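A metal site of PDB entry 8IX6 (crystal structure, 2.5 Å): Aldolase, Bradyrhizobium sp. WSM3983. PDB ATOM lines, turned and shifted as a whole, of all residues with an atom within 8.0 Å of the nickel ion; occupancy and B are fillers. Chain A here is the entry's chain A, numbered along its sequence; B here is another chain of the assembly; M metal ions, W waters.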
ATOM      1  N   LEU A  50     -23.218  -4.066  33.559  1.00  0.00           N
ATOM      2  CA  LEU A  50     -22.325  -3.799  34.678  1.00  0.00           C
ATOM      3  C   LEU A  50     -20.855  -3.831  34.257  1.00  0.00           C
ATOM      4  O   LEU A  50     -19.983  -4.040  35.102  1.00  0.00           O
ATOM      5  CB  LEU A  50     -22.577  -4.796  35.806  1.00  0.00           C
ATOM      6  CG  LEU A  50     -24.016  -4.846  36.323  1.00  0.00           C
ATOM      7  CD1 LEU A  50     -24.258  -6.094  37.166  1.00  0.00           C
ATOM      8  CD2 LEU A  50     -24.349  -3.594  37.123  1.00  0.00           C
ATOM      9  N   ALA A  51     -20.572  -3.634  32.964  1.00  0.00           N
ATOM     10  CA  ALA A  51     -19.196  -3.618  32.494  1.00  0.00           C
ATOM     11  C   ALA A  51     -18.454  -2.362  32.913  1.00  0.00           C
ATOM     12  O   ALA A  51     -17.221  -2.380  32.980  1.00  0.00           O
ATOM     13  CB  ALA A  51     -19.165  -3.764  30.970  1.00  0.00           C
ATOM     14  N   GLY A  52     -19.172  -1.268  33.188  1.00  0.00           N
ATOM     15  CA  GLY A  52     -18.550  -0.025  33.574  1.00  0.00           C
ATOM     16  C   GLY A  52     -17.727  -0.131  34.842  1.00  0.00           C
ATOM     17  O   GLY A  52     -18.206  -0.632  35.865  1.00  0.00           O
ATOM     18  N   GLN A  53     -16.478   0.332  34.786  1.00  0.00           N
ATOM     19  CA  GLN A  53     -15.568   0.305  35.921  1.00  0.00           C
ATOM     20  C   GLN A  53     -14.929   1.673  36.101  1.00  0.00           C
ATOM     21  O   GLN A  53     -14.542   2.322  35.130  1.00  0.00           O
ATOM     22  CB  GLN A  53     -14.470  -0.753  35.732  1.00  0.00           C
ATOM     23  CG  GLN A  53     -14.979  -2.132  35.354  1.00  0.00           C
ATOM     24  CD  GLN A  53     -13.847  -3.069  34.971  1.00  0.00           C
ATOM     25  OE1 GLN A  53     -12.691  -2.670  34.892  1.00  0.00           O
ATOM     26  NE2 GLN A  53     -14.193  -4.329  34.724  1.00  0.00           N
ATOM     27  N   ALA A 100     -13.636  -7.617  38.424  1.00  0.00           N
ATOM     28  CA  ALA A 100     -13.004  -7.333  37.143  1.00  0.00           C
ATOM     29  C   ALA A 100     -12.202  -6.037  37.167  1.00  0.00           C
ATOM     30  O   ALA A 100     -11.536  -5.722  36.166  1.00  0.00           O
ATOM     31  CB  ALA A 100     -14.061  -7.268  36.039  1.00  0.00           C
ATOM     32  N   PHE A 103      -7.445  -5.652  37.964  1.00  0.00           N
ATOM     33  CA  PHE A 103      -6.314  -5.302  37.102  1.00  0.00           C
ATOM     34  C   PHE A 103      -5.967  -3.817  37.172  1.00  0.00           C
ATOM     35  O   PHE A 103      -4.913  -3.432  36.655  1.00  0.00           O
ATOM     36  CB  PHE A 103      -6.613  -5.698  35.660  1.00  0.00           C
ATOM     37  CG  PHE A 103      -7.453  -4.701  34.901  1.00  0.00           C
ATOM     38  CD1 PHE A 103      -8.837  -4.751  34.973  1.00  0.00           C
ATOM     39  CD2 PHE A 103      -6.863  -3.726  34.110  1.00  0.00           C
ATOM     40  CE1 PHE A 103      -9.619  -3.839  34.279  1.00  0.00           C
ATOM     41  CE2 PHE A 103      -7.634  -2.812  33.423  1.00  0.00           C
ATOM     42  CZ  PHE A 103      -9.012  -2.867  33.501  1.00  0.00           C
ATOM     43  N   HIS A 119     -12.981   2.398  32.692  1.00  0.00           N
ATOM     44  CA  HIS A 119     -13.075   1.415  31.620  1.00  0.00           C
ATOM     45  C   HIS A 119     -14.534   1.053  31.413  1.00  0.00           C
ATOM     46  O   HIS A 119     -15.169   0.504  32.319  1.00  0.00           O
ATOM     47  CB  HIS A 119     -12.249   0.161  31.934  1.00  0.00           C
ATOM     48  CG  HIS A 119     -12.759  -1.074  31.246  1.00  0.00           C
ATOM     49  ND1 HIS A 119     -12.656  -1.267  29.881  1.00  0.00           N
ATOM     50  CD2 HIS A 119     -13.383  -2.169  31.738  1.00  0.00           C
ATOM     51  CE1 HIS A 119     -13.182  -2.431  29.563  1.00  0.00           C
ATOM     52  NE2 HIS A 119     -13.641  -3.002  30.671  1.00  0.00           N
ATOM     53  N   THR A 120     -15.074   1.381  30.240  1.00  0.00           N
ATOM     54  CA  THR A 120     -16.453   1.064  29.908  1.00  0.00           C
ATOM     55  C   THR A 120     -16.517   0.464  28.510  1.00  0.00           C
ATOM     56  O   THR A 120     -15.571   0.563  27.721  1.00  0.00           O
ATOM     57  CB  THR A 120     -17.375   2.287  29.962  1.00  0.00           C
ATOM     58  OG1 THR A 120     -17.236   3.048  28.761  1.00  0.00           O
ATOM     59  CG2 THR A 120     -17.037   3.164  31.149  1.00  0.00           C
ATOM     60  N   HIS A 121     -17.646  -0.172  28.210  1.00  0.00           N
ATOM     61  CA  HIS A 121     -17.919  -0.657  26.863  1.00  0.00           C
ATOM     62  C   HIS A 121     -18.951   0.236  26.195  1.00  0.00           C
ATOM     63  O   HIS A 121     -20.004  -0.245  25.765  1.00  0.00           O
ATOM     64  CB  HIS A 121     -18.420  -2.109  26.896  1.00  0.00           C
ATOM     65  CG  HIS A 121     -17.524  -3.048  27.657  1.00  0.00           C
ATOM     66  ND1 HIS A 121     -17.798  -4.398  27.756  1.00  0.00           N
ATOM     67  CD2 HIS A 121     -16.372  -2.847  28.333  1.00  0.00           C
ATOM     68  CE1 HIS A 121     -16.854  -4.978  28.481  1.00  0.00           C
ATOM     69  NE2 HIS A 121     -15.976  -4.061  28.833  1.00  0.00           N
ATOM     70  N   TRP A 155      -7.020  -8.945  21.677  1.00  0.00           N
ATOM     71  CA  TRP A 155      -8.104  -9.126  22.631  1.00  0.00           C
ATOM     72  C   TRP A 155      -7.869 -10.416  23.378  1.00  0.00           C
ATOM     73  O   TRP A 155      -7.998 -11.500  22.786  1.00  0.00           O
ATOM     74  CB  TRP A 155      -9.457  -9.152  21.917  1.00  0.00           C
ATOM     75  CG  TRP A 155     -10.570  -9.489  22.846  1.00  0.00           C
ATOM     76  CD1 TRP A 155     -10.979  -8.772  23.935  1.00  0.00           C
ATOM     77  CD2 TRP A 155     -11.430 -10.638  22.783  1.00  0.00           C
ATOM     78  NE1 TRP A 155     -12.035  -9.394  24.546  1.00  0.00           N
ATOM     79  CE2 TRP A 155     -12.331 -10.546  23.863  1.00  0.00           C
ATOM     80  CE3 TRP A 155     -11.526 -11.731  21.919  1.00  0.00           C
ATOM     81  CZ2 TRP A 155     -13.320 -11.504  24.095  1.00  0.00           C
ATOM     82  CZ3 TRP A 155     -12.491 -12.683  22.151  1.00  0.00           C
ATOM     83  CH2 TRP A 155     -13.379 -12.562  23.229  1.00  0.00           C
ATOM     84  N   GLY A 157      -9.515 -12.130  25.581  1.00  0.00           N
ATOM     85  CA  GLY A 157     -10.635 -12.902  26.071  1.00  0.00           C
ATOM     86  C   GLY A 157     -11.019 -12.534  27.483  1.00  0.00           C
ATOM     87  O   GLY A 157     -11.320 -11.370  27.770  1.00  0.00           O
ATOM     88  N   GLU A 164      -4.366  -9.437  32.146  1.00  0.00           N
ATOM     89  CA  GLU A 164      -5.057  -8.242  31.666  1.00  0.00           C
ATOM     90  C   GLU A 164      -4.373  -6.975  32.155  1.00  0.00           C
ATOM     91  O   GLU A 164      -4.240  -6.006  31.405  1.00  0.00           O
ATOM     92  CB  GLU A 164      -6.523  -8.271  32.110  1.00  0.00           C
ATOM     93  CG  GLU A 164      -7.137  -6.906  32.292  1.00  0.00           C
ATOM     94  CD  GLU A 164      -8.648  -6.942  32.208  1.00  0.00           C
ATOM     95  OE1 GLU A 164      -9.286  -7.529  33.113  1.00  0.00           O
ATOM     96  OE2 GLU A 164      -9.206  -6.384  31.237  1.00  0.00           O
ATOM     97  N   ILE A 168      -2.442  -4.334  29.408  1.00  0.00           N
ATOM     98  CA  ILE A 168      -2.904  -2.957  29.214  1.00  0.00           C
ATOM     99  C   ILE A 168      -1.825  -1.972  29.641  1.00  0.00           C
ATOM    100  O   ILE A 168      -1.639  -0.932  28.997  1.00  0.00           O
ATOM    101  CB  ILE A 168      -4.227  -2.737  29.977  1.00  0.00           C
ATOM    102  CG1 ILE A 168      -5.292  -3.709  29.479  1.00  0.00           C
ATOM    103  CG2 ILE A 168      -4.705  -1.298  29.812  1.00  0.00           C
ATOM    104  CD1 ILE A 168      -6.668  -3.480  30.059  1.00  0.00           C
ATOM    105  N   LEU A 180      -9.141  -0.706  23.374  1.00  0.00           N
ATOM    106  CA  LEU A 180      -8.925  -2.144  23.512  1.00  0.00           C
ATOM    107  C   LEU A 180      -9.744  -2.847  22.434  1.00  0.00           C
ATOM    108  O   LEU A 180     -10.975  -2.867  22.503  1.00  0.00           O
ATOM    109  CB  LEU A 180      -9.317  -2.622  24.911  1.00  0.00           C
ATOM    110  CG  LEU A 180      -8.756  -1.750  26.040  1.00  0.00           C
ATOM    111  CD1 LEU A 180      -9.589  -1.890  27.306  1.00  0.00           C
ATOM    112  CD2 LEU A 180      -7.290  -2.089  26.315  1.00  0.00           C
ATOM    113  N   HIS A 182     -11.858  -5.167  20.097  1.00  0.00           N
ATOM    114  CA  HIS A 182     -12.921  -6.113  20.402  1.00  0.00           C
ATOM    115  C   HIS A 182     -13.407  -6.007  21.843  1.00  0.00           C
ATOM    116  O   HIS A 182     -13.931  -6.973  22.401  1.00  0.00           O
ATOM    117  CB  HIS A 182     -12.482  -7.564  20.118  1.00  0.00           C
ATOM    118  CG  HIS A 182     -11.813  -7.737  18.788  1.00  0.00           C
ATOM    119  ND1 HIS A 182     -12.493  -7.671  17.597  1.00  0.00           N
ATOM    120  CD2 HIS A 182     -10.524  -8.002  18.474  1.00  0.00           C
ATOM    121  CE1 HIS A 182     -11.651  -7.871  16.592  1.00  0.00           C
ATOM    122  NE2 HIS A 182     -10.449  -8.078  17.099  1.00  0.00           N
ATOM    123  N   HIS A 183     -13.259  -4.839  22.467  1.00  0.00           N
ATOM    124  CA  HIS A 183     -13.548  -4.710  23.887  1.00  0.00           C
ATOM    125  C   HIS A 183     -14.164  -3.353  24.205  1.00  0.00           C
ATOM    126  O   HIS A 183     -15.388  -3.231  24.340  1.00  0.00           O
ATOM    127  CB  HIS A 183     -12.278  -4.932  24.698  1.00  0.00           C
ATOM    128  CG  HIS A 183     -12.518  -5.115  26.173  1.00  0.00           C
ATOM    129  ND1 HIS A 183     -11.497  -5.159  27.087  1.00  0.00           N
ATOM    130  CD2 HIS A 183     -13.660  -5.259  26.869  1.00  0.00           C
ATOM    131  CE1 HIS A 183     -12.000  -5.329  28.297  1.00  0.00           C
ATOM    132  NE2 HIS A 183     -13.316  -5.394  28.196  1.00  0.00           N
ATOM    133  N   GLY A 184     -13.309  -2.340  24.326  1.00  0.00           N
ATOM    134  CA  GLY A 184     -13.765  -0.998  24.638  1.00  0.00           C
ATOM    135  C   GLY A 184     -12.600  -0.032  24.745  1.00  0.00           C
ATOM    136  O   GLY A 184     -11.730  -0.013  23.864  1.00  0.00           O
ATOM    137  N   TYR A 185     -12.566   0.751  25.814  1.00  0.00           N
ATOM    138  CA  TYR A 185     -11.481   1.699  26.038  1.00  0.00           C
ATOM    139  C   TYR A 185     -11.154   1.763  27.517  1.00  0.00           C
ATOM    140  O   TYR A 185     -11.848   1.182  28.361  1.00  0.00           O
ATOM    141  CB  TYR A 185     -11.843   3.098  25.517  1.00  0.00           C
ATOM    142  CG  TYR A 185     -12.810   3.840  26.413  1.00  0.00           C
ATOM    143  CD1 TYR A 185     -14.181   3.667  26.292  1.00  0.00           C
ATOM    144  CD2 TYR A 185     -12.347   4.726  27.392  1.00  0.00           C
ATOM    145  CE1 TYR A 185     -15.060   4.335  27.109  1.00  0.00           C
ATOM    146  CE2 TYR A 185     -13.225   5.391  28.223  1.00  0.00           C
ATOM    147  CZ  TYR A 185     -14.581   5.195  28.081  1.00  0.00           C
ATOM    148  OH  TYR A 185     -15.472   5.861  28.892  1.00  0.00           O
ATOM    149  N   GLN B 139     -16.844  -8.291  19.232  1.00  0.00           N
ATOM    150  CA  GLN B 139     -16.602  -7.508  20.441  1.00  0.00           C
ATOM    151  C   GLN B 139     -17.070  -8.323  21.642  1.00  0.00           C
ATOM    152  O   GLN B 139     -17.890  -9.233  21.520  1.00  0.00           O
ATOM    153  CB  GLN B 139     -17.323  -6.156  20.366  1.00  0.00           C
ATOM    154  CG  GLN B 139     -16.933  -5.161  21.445  1.00  0.00           C
ATOM    155  CD  GLN B 139     -17.904  -5.167  22.602  1.00  0.00           C
ATOM    156  OE1 GLN B 139     -18.991  -5.755  22.520  1.00  0.00           O
ATOM    157  NE2 GLN B 139     -17.533  -4.513  23.704  1.00  0.00           N
ATOM    158  N   MET B 140     -16.523  -7.984  22.804  1.00  0.00           N
ATOM    159  CA  MET B 140     -16.706  -8.802  24.010  1.00  0.00           C
ATOM    160  C   MET B 140     -18.178  -8.992  24.347  1.00  0.00           C
ATOM    161  O   MET B 140     -18.622 -10.111  24.628  1.00  0.00           O
ATOM    162  CB  MET B 140     -15.961  -8.170  25.179  1.00  0.00           C
ATOM    163  CG  MET B 140     -16.511  -8.549  26.543  1.00  0.00           C
ATOM    164  SD  MET B 140     -15.674  -9.981  27.246  1.00  0.00           S
ATOM    165  CE  MET B 140     -13.985  -9.408  27.238  1.00  0.00           C
ATOM    166  N   ASP B 141     -18.953  -7.905  24.320  1.00  0.00           N
ATOM    167  CA  ASP B 141     -20.366  -8.003  24.674  1.00  0.00           C
ATOM    168  C   ASP B 141     -21.196  -8.757  23.643  1.00  0.00           C
ATOM    169  O   ASP B 141     -22.382  -8.971  23.871  1.00  0.00           O
ATOM    170  CB  ASP B 141     -20.947  -6.606  24.890  1.00  0.00           C
ATOM    171  CG  ASP B 141     -20.407  -5.936  26.151  1.00  0.00           C
ATOM    172  OD1 ASP B 141     -20.370  -6.586  27.213  1.00  0.00           O
ATOM    173  OD2 ASP B 141     -20.009  -4.757  26.066  1.00  0.00           O
ATOM    174  N   TYR B 232     -18.352 -16.887  30.327  1.00  0.00           N
ATOM    175  CA  TYR B 232     -18.229 -15.980  31.468  1.00  0.00           C
ATOM    176  C   TYR B 232     -19.404 -15.009  31.542  1.00  0.00           C
ATOM    177  O   TYR B 232     -19.916 -14.729  32.624  1.00  0.00           O
ATOM    178  CB  TYR B 232     -16.904 -15.211  31.400  1.00  0.00           C
ATOM    179  CG  TYR B 232     -16.837 -14.043  32.354  1.00  0.00           C
ATOM    180  CD1 TYR B 232     -16.599 -14.239  33.710  1.00  0.00           C
ATOM    181  CD2 TYR B 232     -17.003 -12.740  31.902  1.00  0.00           C
ATOM    182  CE1 TYR B 232     -16.531 -13.163  34.586  1.00  0.00           C
ATOM    183  CE2 TYR B 232     -16.941 -11.659  32.773  1.00  0.00           C
ATOM    184  CZ  TYR B 232     -16.700 -11.882  34.116  1.00  0.00           C
ATOM    185  OH  TYR B 232     -16.634 -10.817  34.983  1.00  0.00           O
HETATM  186 NI    NI M   1     -14.360  -4.815  29.924  1.00  0.00          NI
HETATM  187  O   HOH W   1     -15.532  -4.980  32.203  1.00  0.00           O
HETATM  188  O   HOH W   2     -12.807  -5.553  31.484  1.00  0.00           O
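O of His 119 lies within hydrogen-bond range of N of Gln 53 (2.8 Å).
The backbone carbonyl oxygen (O) of Tyr 185 lies within hydrogen-bond range of a ring nitrogen (ND1) of His 119.
OD2 of Asp 141 of chain B sits at hydrogen-bond distance from ND1 of His 121 (2.8 Å).
The backbone carbonyl oxygen (O) of His 183 sits at hydrogen-bond distance from the side-chain amide nitrogen (NE2) of Gln 139 of chain B (2.6 Å).
Three residues have an atom within 4 Å of the nickel ion: His 119, His 121 and His 183.
The nickel ion is bound by NE2 of His 119 (2.1 Å), NE2 of His 121 (2.1 Å), NE2 of His 183 (2.1 Å), water W2 (2.3 Å) and water W1 (2.6 Å).
The nickel ion has five donor atoms within binding distance.
Water W1 lies within hydrogen-bond range of the side-chain amide nitrogen (NE2) of Gln 53 and the backbone carbonyl oxygen (O) of Ala 51.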
